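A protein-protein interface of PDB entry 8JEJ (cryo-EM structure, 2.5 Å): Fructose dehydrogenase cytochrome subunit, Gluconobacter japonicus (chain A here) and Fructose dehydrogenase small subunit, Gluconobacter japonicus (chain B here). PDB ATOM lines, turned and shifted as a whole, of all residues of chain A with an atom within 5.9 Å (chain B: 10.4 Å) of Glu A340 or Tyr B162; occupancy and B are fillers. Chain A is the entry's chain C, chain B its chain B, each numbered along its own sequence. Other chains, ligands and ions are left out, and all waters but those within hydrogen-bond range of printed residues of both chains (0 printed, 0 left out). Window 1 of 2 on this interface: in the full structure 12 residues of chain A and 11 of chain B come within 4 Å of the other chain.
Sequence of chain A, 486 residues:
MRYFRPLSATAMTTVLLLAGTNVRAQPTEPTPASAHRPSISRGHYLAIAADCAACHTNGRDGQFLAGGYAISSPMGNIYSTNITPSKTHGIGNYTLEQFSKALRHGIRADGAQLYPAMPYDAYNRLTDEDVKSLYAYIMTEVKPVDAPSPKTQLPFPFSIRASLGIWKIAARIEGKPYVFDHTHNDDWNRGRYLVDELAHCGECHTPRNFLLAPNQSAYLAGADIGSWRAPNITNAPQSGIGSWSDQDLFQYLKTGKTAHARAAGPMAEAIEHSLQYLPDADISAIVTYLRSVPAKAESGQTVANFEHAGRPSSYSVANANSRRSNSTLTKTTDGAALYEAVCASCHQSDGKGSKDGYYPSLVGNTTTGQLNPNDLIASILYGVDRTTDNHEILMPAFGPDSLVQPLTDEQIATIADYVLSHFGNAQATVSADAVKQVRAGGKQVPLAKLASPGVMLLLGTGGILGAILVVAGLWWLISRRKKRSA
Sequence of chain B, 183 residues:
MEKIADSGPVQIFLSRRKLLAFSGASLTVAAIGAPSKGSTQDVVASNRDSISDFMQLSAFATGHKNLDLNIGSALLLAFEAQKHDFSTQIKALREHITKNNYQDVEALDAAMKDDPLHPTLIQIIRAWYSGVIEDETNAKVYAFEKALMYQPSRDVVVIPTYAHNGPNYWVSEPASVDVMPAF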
ATOM      1  N   SER A 314      13.621  -8.099  16.924  1.00  0.00           N
ATOM      2  CA  SER A 314      14.772  -8.733  16.295  1.00  0.00           C
ATOM      3  C   SER A 314      14.753  -8.427  14.796  1.00  0.00           C
ATOM      4  O   SER A 314      14.058  -7.509  14.348  1.00  0.00           O
ATOM      5  CB  SER A 314      14.786 -10.240  16.601  1.00  0.00           C
ATOM      6  OG  SER A 314      15.258 -10.474  17.916  1.00  0.00           O
ATOM      7  N   TYR A 315      15.533  -9.189  14.032  1.00  0.00           N
ATOM      8  CA  TYR A 315      15.742  -8.938  12.615  1.00  0.00           C
ATOM      9  C   TYR A 315      14.758  -9.764  11.785  1.00  0.00           C
ATOM     10  O   TYR A 315      13.863 -10.426  12.315  1.00  0.00           O
ATOM     11  CB  TYR A 315      17.214  -9.194  12.272  1.00  0.00           C
ATOM     12  CG  TYR A 315      17.575 -10.523  11.641  1.00  0.00           C
ATOM     13  CD1 TYR A 315      17.149 -11.730  12.187  1.00  0.00           C
ATOM     14  CD2 TYR A 315      18.384 -10.566  10.515  1.00  0.00           C
ATOM     15  CE1 TYR A 315      17.494 -12.932  11.606  1.00  0.00           C
ATOM     16  CE2 TYR A 315      18.735 -11.760   9.932  1.00  0.00           C
ATOM     17  CZ  TYR A 315      18.289 -12.940  10.480  1.00  0.00           C
ATOM     18  OH  TYR A 315      18.642 -14.131   9.894  1.00  0.00           O
ATOM     19  N   GLY A 335      21.042  -2.511  11.272  1.00  0.00           N
ATOM     20  CA  GLY A 335      21.678  -2.836  12.538  1.00  0.00           C
ATOM     21  C   GLY A 335      21.312  -4.217  13.041  1.00  0.00           C
ATOM     22  O   GLY A 335      22.161  -4.941  13.567  1.00  0.00           O
ATOM     23  N   ALA A 336      20.043  -4.599  12.896  1.00  0.00           N
ATOM     24  CA  ALA A 336      19.614  -5.929  13.312  1.00  0.00           C
ATOM     25  C   ALA A 336      20.292  -7.013  12.484  1.00  0.00           C
ATOM     26  O   ALA A 336      20.732  -8.034  13.026  1.00  0.00           O
ATOM     27  CB  ALA A 336      18.095  -6.036  13.207  1.00  0.00           C
ATOM     28  N   ALA A 337      20.391  -6.807  11.170  1.00  0.00           N
ATOM     29  CA  ALA A 337      21.053  -7.783  10.310  1.00  0.00           C
ATOM     30  C   ALA A 337      22.535  -7.900  10.643  1.00  0.00           C
ATOM     31  O   ALA A 337      23.083  -9.008  10.689  1.00  0.00           O
ATOM     32  CB  ALA A 337      20.860  -7.404   8.842  1.00  0.00           C
ATOM     33  N   LEU A 338      23.200  -6.766  10.874  1.00  0.00           N
ATOM     34  CA  LEU A 338      24.611  -6.796  11.241  1.00  0.00           C
ATOM     35  C   LEU A 338      24.821  -7.499  12.576  1.00  0.00           C
ATOM     36  O   LEU A 338      25.755  -8.296  12.727  1.00  0.00           O
ATOM     37  CB  LEU A 338      25.169  -5.375  11.289  1.00  0.00           C
ATOM     38  CG  LEU A 338      25.510  -4.719   9.953  1.00  0.00           C
ATOM     39  CD1 LEU A 338      25.711  -3.228  10.139  1.00  0.00           C
ATOM     40  CD2 LEU A 338      26.747  -5.357   9.348  1.00  0.00           C
ATOM     41  N   TYR A 339      23.962  -7.216  13.559  1.00  0.00           N
ATOM     42  CA  TYR A 339      24.065  -7.898  14.844  1.00  0.00           C
ATOM     43  C   TYR A 339      23.868  -9.398  14.684  1.00  0.00           C
ATOM     44  O   TYR A 339      24.594 -10.193  15.291  1.00  0.00           O
ATOM     45  CB  TYR A 339      23.048  -7.333  15.835  1.00  0.00           C
ATOM     46  CG  TYR A 339      22.935  -8.155  17.101  1.00  0.00           C
ATOM     47  CD1 TYR A 339      23.829  -7.977  18.147  1.00  0.00           C
ATOM     48  CD2 TYR A 339      21.944  -9.117  17.242  1.00  0.00           C
ATOM     49  CE1 TYR A 339      23.736  -8.729  19.297  1.00  0.00           C
ATOM     50  CE2 TYR A 339      21.847  -9.875  18.388  1.00  0.00           C
ATOM     51  CZ  TYR A 339      22.745  -9.677  19.412  1.00  0.00           C
ATOM     52  OH  TYR A 339      22.648 -10.429  20.558  1.00  0.00           O
ATOM     53  N   GLU A 340      22.885  -9.805  13.880  1.00  0.00           N
ATOM     54  CA  GLU A 340      22.655 -11.230  13.677  1.00  0.00           C
ATOM     55  C   GLU A 340      23.849 -11.889  13.002  1.00  0.00           C
ATOM     56  O   GLU A 340      24.225 -13.016  13.348  1.00  0.00           O
ATOM     57  CB  GLU A 340      21.385 -11.451  12.859  1.00  0.00           C
ATOM     58  CG  GLU A 340      20.889 -12.886  12.881  1.00  0.00           C
ATOM     59  CD  GLU A 340      20.012 -13.183  14.079  1.00  0.00           C
ATOM     60  OE1 GLU A 340      19.718 -12.247  14.851  1.00  0.00           O
ATOM     61  OE2 GLU A 340      19.614 -14.352  14.249  1.00  0.00           O
ATOM     62  N   ALA A 341      24.460 -11.202  12.036  1.00  0.00           N
ATOM     63  CA  ALA A 341      25.559 -11.803  11.291  1.00  0.00           C
ATOM     64  C   ALA A 341      26.825 -11.901  12.133  1.00  0.00           C
ATOM     65  O   ALA A 341      27.554 -12.897  12.049  1.00  0.00           O
ATOM     66  CB  ALA A 341      25.822 -11.005  10.016  1.00  0.00           C
ATOM     67  N   VAL A 342      27.106 -10.889  12.953  1.00  0.00           N
ATOM     68  CA  VAL A 342      28.400 -10.798  13.621  1.00  0.00           C
ATOM     69  C   VAL A 342      28.317 -11.255  15.073  1.00  0.00           C
ATOM     70  O   VAL A 342      29.297 -11.762  15.629  1.00  0.00           O
ATOM     71  CB  VAL A 342      28.955  -9.362  13.531  1.00  0.00           C
ATOM     72  CG1 VAL A 342      30.392  -9.307  14.023  1.00  0.00           C
ATOM     73  CG2 VAL A 342      28.869  -8.850  12.103  1.00  0.00           C
ATOM     74  N   CYS A 343      27.154 -11.094  15.698  1.00  0.00           N
ATOM     75  CA  CYS A 343      27.049 -11.261  17.141  1.00  0.00           C
ATOM     76  C   CYS A 343      26.078 -12.334  17.599  1.00  0.00           C
ATOM     77  O   CYS A 343      26.279 -12.892  18.680  1.00  0.00           O
ATOM     78  CB  CYS A 343      26.642  -9.933  17.799  1.00  0.00           C
ATOM     79  SG  CYS A 343      27.388  -8.449  17.071  1.00  0.00           S
ATOM     80  N   ALA A 344      25.039 -12.642  16.821  1.00  0.00           N
ATOM     81  CA  ALA A 344      23.966 -13.501  17.307  1.00  0.00           C
ATOM     82  C   ALA A 344      24.411 -14.929  17.595  1.00  0.00           C
ATOM     83  O   ALA A 344      23.671 -15.661  18.258  1.00  0.00           O
ATOM     84  CB  ALA A 344      22.807 -13.522  16.315  1.00  0.00           C
ATOM     85  N   SER A 345      25.587 -15.345  17.121  1.00  0.00           N
ATOM     86  CA  SER A 345      26.031 -16.717  17.348  1.00  0.00           C
ATOM     87  C   SER A 345      26.245 -16.993  18.831  1.00  0.00           C
ATOM     88  O   SER A 345      25.783 -18.013  19.358  1.00  0.00           O
ATOM     89  CB  SER A 345      27.311 -16.988  16.560  1.00  0.00           C
ATOM     90  OG  SER A 345      27.682 -18.351  16.654  1.00  0.00           O
ATOM     91  N   GLN A 348      22.589 -14.567  21.965  1.00  0.00           N
ATOM     92  CA  GLN A 348      21.536 -15.066  21.096  1.00  0.00           C
ATOM     93  C   GLN A 348      20.831 -13.908  20.386  1.00  0.00           C
ATOM     94  O   GLN A 348      21.156 -12.731  20.569  1.00  0.00           O
ATOM     95  CB  GLN A 348      20.566 -15.923  21.901  1.00  0.00           C
ATOM     96  CG  GLN A 348      21.222 -17.165  22.485  1.00  0.00           C
ATOM     97  CD  GLN A 348      22.124 -17.873  21.488  1.00  0.00           C
ATOM     98  OE1 GLN A 348      21.658 -18.401  20.480  1.00  0.00           O
ATOM     99  NE2 GLN A 348      23.422 -17.887  21.768  1.00  0.00           N
ATOM    100  N   SER A 349      19.861 -14.254  19.535  1.00  0.00           N
ATOM    101  CA  SER A 349      19.145 -13.232  18.777  1.00  0.00           C
ATOM    102  C   SER A 349      18.330 -12.317  19.682  1.00  0.00           C
ATOM    103  O   SER A 349      18.087 -11.159  19.328  1.00  0.00           O
ATOM    104  CB  SER A 349      18.238 -13.885  17.734  1.00  0.00           C
ATOM    105  OG  SER A 349      18.082 -13.043  16.607  1.00  0.00           O
ATOM    106  N   ILE B  71       7.153 -13.718  10.582  1.00  0.00           N
ATOM    107  CA  ILE B  71       7.346 -14.878   9.719  1.00  0.00           C
ATOM    108  C   ILE B  71       6.034 -15.254   9.047  1.00  0.00           C
ATOM    109  O   ILE B  71       6.002 -15.572   7.854  1.00  0.00           O
ATOM    110  CB  ILE B  71       7.934 -16.052  10.524  1.00  0.00           C
ATOM    111  CG1 ILE B  71       9.341 -15.710  11.015  1.00  0.00           C
ATOM    112  CG2 ILE B  71       7.959 -17.319   9.684  1.00  0.00           C
ATOM    113  CD1 ILE B  71       9.928 -16.738  11.954  1.00  0.00           C
ATOM    114  N   VAL B 141      14.359 -18.162   1.960  1.00  0.00           N
ATOM    115  CA  VAL B 141      14.216 -18.693   3.309  1.00  0.00           C
ATOM    116  C   VAL B 141      13.558 -17.627   4.170  1.00  0.00           C
ATOM    117  O   VAL B 141      14.033 -16.487   4.232  1.00  0.00           O
ATOM    118  CB  VAL B 141      15.576 -19.119   3.888  1.00  0.00           C
ATOM    119  CG1 VAL B 141      15.461 -19.398   5.377  1.00  0.00           C
ATOM    120  CG2 VAL B 141      16.097 -20.343   3.158  1.00  0.00           C
ATOM    121  N   ALA B 143      12.433 -18.431   7.544  1.00  0.00           N
ATOM    122  CA  ALA B 143      12.667 -18.717   8.952  1.00  0.00           C
ATOM    123  C   ALA B 143      13.810 -19.708   9.087  1.00  0.00           C
ATOM    124  O   ALA B 143      13.777 -20.785   8.485  1.00  0.00           O
ATOM    125  CB  ALA B 143      11.406 -19.270   9.622  1.00  0.00           C
ATOM    126  N   PHE B 144      14.819 -19.331   9.865  1.00  0.00           N
ATOM    127  CA  PHE B 144      15.866 -20.235  10.314  1.00  0.00           C
ATOM    128  C   PHE B 144      16.059 -20.019  11.805  1.00  0.00           C
ATOM    129  O   PHE B 144      15.991 -18.882  12.284  1.00  0.00           O
ATOM    130  CB  PHE B 144      17.185 -20.004   9.570  1.00  0.00           C
ATOM    131  CG  PHE B 144      18.297 -20.909  10.015  1.00  0.00           C
ATOM    132  CD1 PHE B 144      18.186 -22.282   9.883  1.00  0.00           C
ATOM    133  CD2 PHE B 144      19.454 -20.388  10.567  1.00  0.00           C
ATOM    134  CE1 PHE B 144      19.207 -23.115  10.292  1.00  0.00           C
ATOM    135  CE2 PHE B 144      20.476 -21.218  10.978  1.00  0.00           C
ATOM    136  CZ  PHE B 144      20.352 -22.581  10.839  1.00  0.00           C
ATOM    137  N   GLU B 145      16.246 -21.121  12.537  1.00  0.00           N
ATOM    138  CA  GLU B 145      16.410 -21.138  13.989  1.00  0.00           C
ATOM    139  C   GLU B 145      15.077 -20.850  14.674  1.00  0.00           C
ATOM    140  O   GLU B 145      14.925 -21.059  15.881  1.00  0.00           O
ATOM    141  CB  GLU B 145      17.491 -20.139  14.426  1.00  0.00           C
ATOM    142  CG  GLU B 145      17.777 -20.106  15.916  1.00  0.00           C
ATOM    143  CD  GLU B 145      18.038 -18.705  16.425  1.00  0.00           C
ATOM    144  OE1 GLU B 145      17.761 -17.737  15.684  1.00  0.00           O
ATOM    145  OE2 GLU B 145      18.518 -18.569  17.569  1.00  0.00           O
ATOM    146  N   LYS B 146      14.087 -20.429  13.892  1.00  0.00           N
ATOM    147  CA  LYS B 146      12.713 -20.322  14.347  1.00  0.00           C
ATOM    148  C   LYS B 146      11.786 -21.256  13.593  1.00  0.00           C
ATOM    149  O   LYS B 146      10.607 -21.355  13.951  1.00  0.00           O
ATOM    150  CB  LYS B 146      12.204 -18.879  14.208  1.00  0.00           C
ATOM    151  CG  LYS B 146      12.254 -18.083  15.498  1.00  0.00           C
ATOM    152  CD  LYS B 146      11.371 -16.853  15.420  1.00  0.00           C
ATOM    153  CE  LYS B 146      11.853 -15.768  16.366  1.00  0.00           C
ATOM    154  NZ  LYS B 146      10.806 -15.394  17.353  1.00  0.00           N
ATOM    155  N   ALA B 147      12.285 -21.936  12.564  1.00  0.00           N
ATOM    156  CA  ALA B 147      11.500 -22.931  11.853  1.00  0.00           C
ATOM    157  C   ALA B 147      11.140 -24.078  12.786  1.00  0.00           C
ATOM    158  O   ALA B 147      11.934 -24.483  13.638  1.00  0.00           O
ATOM    159  CB  ALA B 147      12.281 -23.444  10.645  1.00  0.00           C
ATOM    160  N   TYR B 150      13.362 -27.421  13.598  1.00  0.00           N
ATOM    161  CA  TYR B 150      14.525 -27.410  14.471  1.00  0.00           C
ATOM    162  C   TYR B 150      14.157 -27.431  15.947  1.00  0.00           C
ATOM    163  O   TYR B 150      15.040 -27.628  16.786  1.00  0.00           O
ATOM    164  CB  TYR B 150      15.393 -26.182  14.188  1.00  0.00           C
ATOM    165  CG  TYR B 150      16.035 -26.196  12.825  1.00  0.00           C
ATOM    166  CD1 TYR B 150      16.980 -27.155  12.493  1.00  0.00           C
ATOM    167  CD2 TYR B 150      15.691 -25.255  11.867  1.00  0.00           C
ATOM    168  CE1 TYR B 150      17.567 -27.174  11.247  1.00  0.00           C
ATOM    169  CE2 TYR B 150      16.272 -25.266  10.618  1.00  0.00           C
ATOM    170  CZ  TYR B 150      17.210 -26.227  10.315  1.00  0.00           C
ATOM    171  OH  TYR B 150      17.791 -26.241   9.070  1.00  0.00           O
ATOM    172  N   GLN B 151      12.884 -27.242  16.277  1.00  0.00           N
ATOM    173  CA  GLN B 151      12.406 -27.166  17.652  1.00  0.00           C
ATOM    174  C   GLN B 151      12.298 -28.521  18.354  1.00  0.00           C
ATOM    175  O   GLN B 151      12.611 -28.600  19.548  1.00  0.00           O
ATOM    176  CB  GLN B 151      11.049 -26.457  17.693  1.00  0.00           C
ATOM    177  CG  GLN B 151      10.980 -25.188  16.864  1.00  0.00           C
ATOM    178  CD  GLN B 151      12.103 -24.222  17.175  1.00  0.00           C
ATOM    179  OE1 GLN B 151      12.284 -23.816  18.320  1.00  0.00           O
ATOM    180  NE2 GLN B 151      12.861 -23.846  16.155  1.00  0.00           N
ATOM    181  N   ARG B 154      15.703 -29.148  19.891  1.00  0.00           N
ATOM    182  CA  ARG B 154      16.476 -27.989  20.324  1.00  0.00           C
ATOM    183  C   ARG B 154      17.139 -28.208  21.676  1.00  0.00           C
ATOM    184  O   ARG B 154      18.206 -27.643  21.936  1.00  0.00           O
ATOM    185  CB  ARG B 154      15.579 -26.757  20.376  1.00  0.00           C
ATOM    186  CG  ARG B 154      15.783 -25.809  19.225  1.00  0.00           C
ATOM    187  CD  ARG B 154      15.114 -24.485  19.492  1.00  0.00           C
ATOM    188  NE  ARG B 154      16.090 -23.432  19.729  1.00  0.00           N
ATOM    189  CZ  ARG B 154      15.892 -22.153  19.444  1.00  0.00           C
ATOM    190  NH1 ARG B 154      14.758 -21.734  18.907  1.00  0.00           N
ATOM    191  NH2 ARG B 154      16.855 -21.274  19.704  1.00  0.00           N
ATOM    192  N   VAL B 156      18.661 -30.720  22.756  1.00  0.00           N
ATOM    193  CA  VAL B 156      19.858 -31.542  22.625  1.00  0.00           C
ATOM    194  C   VAL B 156      20.756 -31.051  21.496  1.00  0.00           C
ATOM    195  O   VAL B 156      21.957 -30.841  21.690  1.00  0.00           O
ATOM    196  CB  VAL B 156      19.499 -33.032  22.425  1.00  0.00           C
ATOM    197  CG1 VAL B 156      20.739 -33.895  22.566  1.00  0.00           C
ATOM    198  CG2 VAL B 156      18.432 -33.466  23.415  1.00  0.00           C
ATOM    199  N   VAL B 157      20.189 -30.854  20.310  1.00  0.00           N
ATOM    200  CA  VAL B 157      20.963 -30.665  19.086  1.00  0.00           C
ATOM    201  C   VAL B 157      21.129 -29.182  18.796  1.00  0.00           C
ATOM    202  O   VAL B 157      20.201 -28.385  18.983  1.00  0.00           O
ATOM    203  CB  VAL B 157      20.299 -31.394  17.902  1.00  0.00           C
ATOM    204  CG1 VAL B 157      21.138 -31.256  16.642  1.00  0.00           C
ATOM    205  CG2 VAL B 157      20.104 -32.853  18.242  1.00  0.00           C
ATOM    206  N   VAL B 158      22.324 -28.813  18.337  1.00  0.00           N
ATOM    207  CA  VAL B 158      22.623 -27.435  17.979  1.00  0.00           C
ATOM    208  C   VAL B 158      21.936 -27.074  16.668  1.00  0.00           C
ATOM    209  O   VAL B 158      21.870 -27.882  15.732  1.00  0.00           O
ATOM    210  CB  VAL B 158      24.147 -27.243  17.887  1.00  0.00           C
ATOM    211  CG1 VAL B 158      24.751 -28.231  16.899  1.00  0.00           C
ATOM    212  CG2 VAL B 158      24.500 -25.820  17.498  1.00  0.00           C
ATOM    213  N   ILE B 159      21.388 -25.864  16.608  1.00  0.00           N
ATOM    214  CA  ILE B 159      21.036 -25.240  15.337  1.00  0.00           C
ATOM    215  C   ILE B 159      22.314 -24.562  14.861  1.00  0.00           C
ATOM    216  O   ILE B 159      22.677 -23.500  15.385  1.00  0.00           O
ATOM    217  CB  ILE B 159      19.865 -24.258  15.487  1.00  0.00           C
ATOM    218  CG1 ILE B 159      18.678 -24.959  16.148  1.00  0.00           C
ATOM    219  CG2 ILE B 159      19.459 -23.694  14.137  1.00  0.00           C
ATOM    220  CD1 ILE B 159      17.503 -24.057  16.390  1.00  0.00           C
ATOM    221  N   PRO B 160      23.003 -25.127  13.861  1.00  0.00           N
ATOM    222  CA  PRO B 160      24.457 -24.941  13.733  1.00  0.00           C
ATOM    223  C   PRO B 160      25.030 -23.547  13.964  1.00  0.00           C
ATOM    224  O   PRO B 160      25.817 -23.373  14.898  1.00  0.00           O
ATOM    225  CB  PRO B 160      24.716 -25.408  12.298  1.00  0.00           C
ATOM    226  CG  PRO B 160      23.738 -26.525  12.127  1.00  0.00           C
ATOM    227  CD  PRO B 160      22.501 -26.142  12.916  1.00  0.00           C
ATOM    228  N   THR B 161      24.646 -22.548  13.189  1.00  0.00           N
ATOM    229  CA  THR B 161      25.417 -21.309  13.369  1.00  0.00           C
ATOM    230  C   THR B 161      25.086 -20.557  14.665  1.00  0.00           C
ATOM    231  O   THR B 161      25.593 -19.444  14.853  1.00  0.00           O
ATOM    232  CB  THR B 161      25.212 -20.384  12.173  1.00  0.00           C
ATOM    233  OG1 THR B 161      23.850 -20.465  11.740  1.00  0.00           O
ATOM    234  CG2 THR B 161      26.130 -20.786  11.033  1.00  0.00           C
ATOM    235  N   TYR B 162      24.267 -21.122  15.546  1.00  0.00           N
ATOM    236  CA  TYR B 162      23.944 -20.530  16.833  1.00  0.00           C
ATOM    237  C   TYR B 162      24.357 -21.493  17.935  1.00  0.00           C
ATOM    238  O   TYR B 162      24.122 -22.700  17.837  1.00  0.00           O
ATOM    239  CB  TYR B 162      22.452 -20.209  16.941  1.00  0.00           C
ATOM    240  CG  TYR B 162      21.980 -19.199  15.925  1.00  0.00           C
ATOM    241  CD1 TYR B 162      21.571 -19.598  14.660  1.00  0.00           C
ATOM    242  CD2 TYR B 162      21.946 -17.845  16.227  1.00  0.00           C
ATOM    243  CE1 TYR B 162      21.144 -18.680  13.728  1.00  0.00           C
ATOM    244  CE2 TYR B 162      21.518 -16.919  15.301  1.00  0.00           C
ATOM    245  CZ  TYR B 162      21.117 -17.343  14.053  1.00  0.00           C
ATOM    246  OH  TYR B 162      20.690 -16.426  13.123  1.00  0.00           O
ATOM    247  N   ALA B 163      24.967 -20.954  18.983  1.00  0.00           N
ATOM    248  CA  ALA B 163      25.597 -21.780  19.999  1.00  0.00           C
ATOM    249  C   ALA B 163      24.594 -22.284  21.028  1.00  0.00           C
ATOM    250  O   ALA B 163      23.695 -21.555  21.457  1.00  0.00           O
ATOM    251  CB  ALA B 163      26.698 -20.994  20.709  1.00  0.00           C
ATOM    252  N   HIS B 164      24.750 -23.550  21.409  1.00  0.00           N
ATOM    253  CA  HIS B 164      24.229 -24.034  22.676  1.00  0.00           C
ATOM    254  C   HIS B 164      25.070 -23.454  23.814  1.00  0.00           C
ATOM    255  O   HIS B 164      26.072 -22.767  23.596  1.00  0.00           O
ATOM    256  CB  HIS B 164      24.243 -25.560  22.710  1.00  0.00           C
ATOM    257  CG  HIS B 164      22.922 -26.194  22.415  1.00  0.00           C
ATOM    258  ND1 HIS B 164      22.194 -26.873  23.369  1.00  0.00           N
ATOM    259  CD2 HIS B 164      22.198 -26.261  21.273  1.00  0.00           C
ATOM    260  CE1 HIS B 164      21.079 -27.327  22.829  1.00  0.00           C
ATOM    261  NE2 HIS B 164      21.056 -26.968  21.558  1.00  0.00           N
ATOM    262  N   ASN B 165      24.682 -23.752  25.049  1.00  0.00           N
ATOM    263  CA  ASN B 165      25.306 -23.073  26.177  1.00  0.00           C
ATOM    264  C   ASN B 165      26.722 -23.562  26.462  1.00  0.00           C
ATOM    265  O   ASN B 165      26.913 -24.538  27.194  1.00  0.00           O
ATOM    266  CB  ASN B 165      24.442 -23.226  27.431  1.00  0.00           C
ATOM    267  CG  ASN B 165      24.027 -24.654  27.682  1.00  0.00           C
ATOM    268  OD1 ASN B 165      24.278 -25.537  26.864  1.00  0.00           O
ATOM    269  ND2 ASN B 165      23.390 -24.893  28.819  1.00  0.00           N
ATOM    270  N   GLY B 166      27.724 -22.888  25.903  1.00  0.00           N
ATOM    271  CA  GLY B 166      29.080 -23.042  26.375  1.00  0.00           C
ATOM    272  C   GLY B 166      30.014 -23.812  25.467  1.00  0.00           C
ATOM    273  O   GLY B 166      29.612 -24.708  24.718  1.00  0.00           O
ATOM    274  N   TYR B 169      29.759 -27.830  26.287  1.00  0.00           N
ATOM    275  CA  TYR B 169      28.508 -28.339  26.842  1.00  0.00           C
ATOM    276  C   TYR B 169      28.280 -29.812  26.528  1.00  0.00           C
ATOM    277  O   TYR B 169      27.541 -30.480  27.260  1.00  0.00           O
ATOM    278  CB  TYR B 169      27.328 -27.507  26.327  1.00  0.00           C
ATOM    279  CG  TYR B 169      26.949 -27.774  24.886  1.00  0.00           C
ATOM    280  CD1 TYR B 169      26.037 -28.770  24.559  1.00  0.00           C
ATOM    281  CD2 TYR B 169      27.499 -27.030  23.853  1.00  0.00           C
ATOM    282  CE1 TYR B 169      25.693 -29.023  23.252  1.00  0.00           C
ATOM    283  CE2 TYR B 169      27.160 -27.275  22.540  1.00  0.00           C
ATOM    284  CZ  TYR B 169      26.256 -28.273  22.246  1.00  0.00           C
ATOM    285  OH  TYR B 169      25.907 -28.523  20.940  1.00  0.00           O
ATOM    286  N   TRP B 170      28.899 -30.337  25.473  1.00  0.00           N
ATOM    287  CA  TRP B 170      28.580 -31.668  24.975  1.00  0.00           C
ATOM    288  C   TRP B 170      29.166 -32.795  25.815  1.00  0.00           C
ATOM    289  O   TRP B 170      29.030 -33.960  25.430  1.00  0.00           O
ATOM    290  CB  TRP B 170      29.055 -31.813  23.529  1.00  0.00           C
ATOM    291  CG  TRP B 170      30.436 -31.307  23.296  1.00  0.00           C
ATOM    292  CD1 TRP B 170      31.603 -31.989  23.473  1.00  0.00           C
ATOM    293  CD2 TRP B 170      30.799 -30.006  22.837  1.00  0.00           C
ATOM    294  NE1 TRP B 170      32.670 -31.190  23.152  1.00  0.00           N
ATOM    295  CE2 TRP B 170      32.202 -29.966  22.759  1.00  0.00           C
ATOM    296  CE3 TRP B 170      30.072 -28.868  22.484  1.00  0.00           C
ATOM    297  CZ2 TRP B 170      32.891 -28.833  22.343  1.00  0.00           C
ATOM    298  CZ3 TRP B 170      30.757 -27.747  22.075  1.00  0.00           C
ATOM    299  CH2 TRP B 170      32.151 -27.738  22.000  1.00  0.00           C
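The backbone carbonyl oxygen of Thr B161 sits at hydrogen-bond distance from the side-chain hydroxyl of Ser A345. OH of Tyr B162 sits at hydrogen-bond distance from OE2 of Glu A340 (2.6 Å). N of Ala B163 sits at hydrogen-bond distance from O of Ser A345 (3.1 Å).
The backbone NH of Ala A344 is in hydrogen-bond range of the backbone carbonyl oxygen of Tyr A339, at 2.9 Å. The side-chain hydroxyl of Tyr A339 is in hydrogen-bond range of the backbone carbonyl oxygen of Gln A348, at 2.7 Å. OG of Ser A349 sits at hydrogen-bond distance from OE1 of Glu A340 (2.5 Å). O of Ser A345 sits at hydrogen-bond distance from NE2 of Gln A348.
O of Ala A344 touches CD2 of Tyr B162, at 3.4 Å. Gln A348 touches Ala B163 (NE2 to O, 3.7 Å).
No residue of chain B comes within 4 Å of Ala A336. Glu A340 touches just one residue of chain B: Tyr B162 (2.6 Å). No residue of chain B comes within 4 Å of Ala A341. No residue of chain B comes within 4 Å of Cys A343. Printed residues of chain B within 4 Å of Ser A345: Thr B161 and Ala B163. Ser A349 touches none of the printed residues of chain B. Arg B154 touches none of the printed residues of chain A. Val B157 touches none of the printed residues of chain A. Of the printed residues of chain A, Thr B161 touches Ser A345. Of the printed residues of chain A, Ala B163 touches Ser A345 (3.1 Å) and Gln A348 (3.7 Å). The nearest residue of chain B that does not touch Glu A340 is Glu B145 (4.1 Å). The nearest printed residue of chain A that does not touch Tyr B162 is Ser A345 (4.01 Å). The nearest printed residue of chain A that does not touch Ala B163 is Ala A344 (5.5 Å).
Of the 15 printed residues of chain A, 4 touch a printed residue of chain B. Printed residues of chain A that touch a printed residue of chain B: Glu A340, Ala A344, Ser A345 and Gln A348. Hydrophobic or aromatic side chains of chain A within 4 Å of the printed part of chain B: Ala A344. Of the 23 printed residues of chain B, 3 touch a printed residue of chain A. Among the printed residues, 5 pairs touch across the chains. Among the printed residues, no Asp or Glu carboxylate lies within 4 Å of a Lys or Arg side-chain nitrogen of the other chain.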
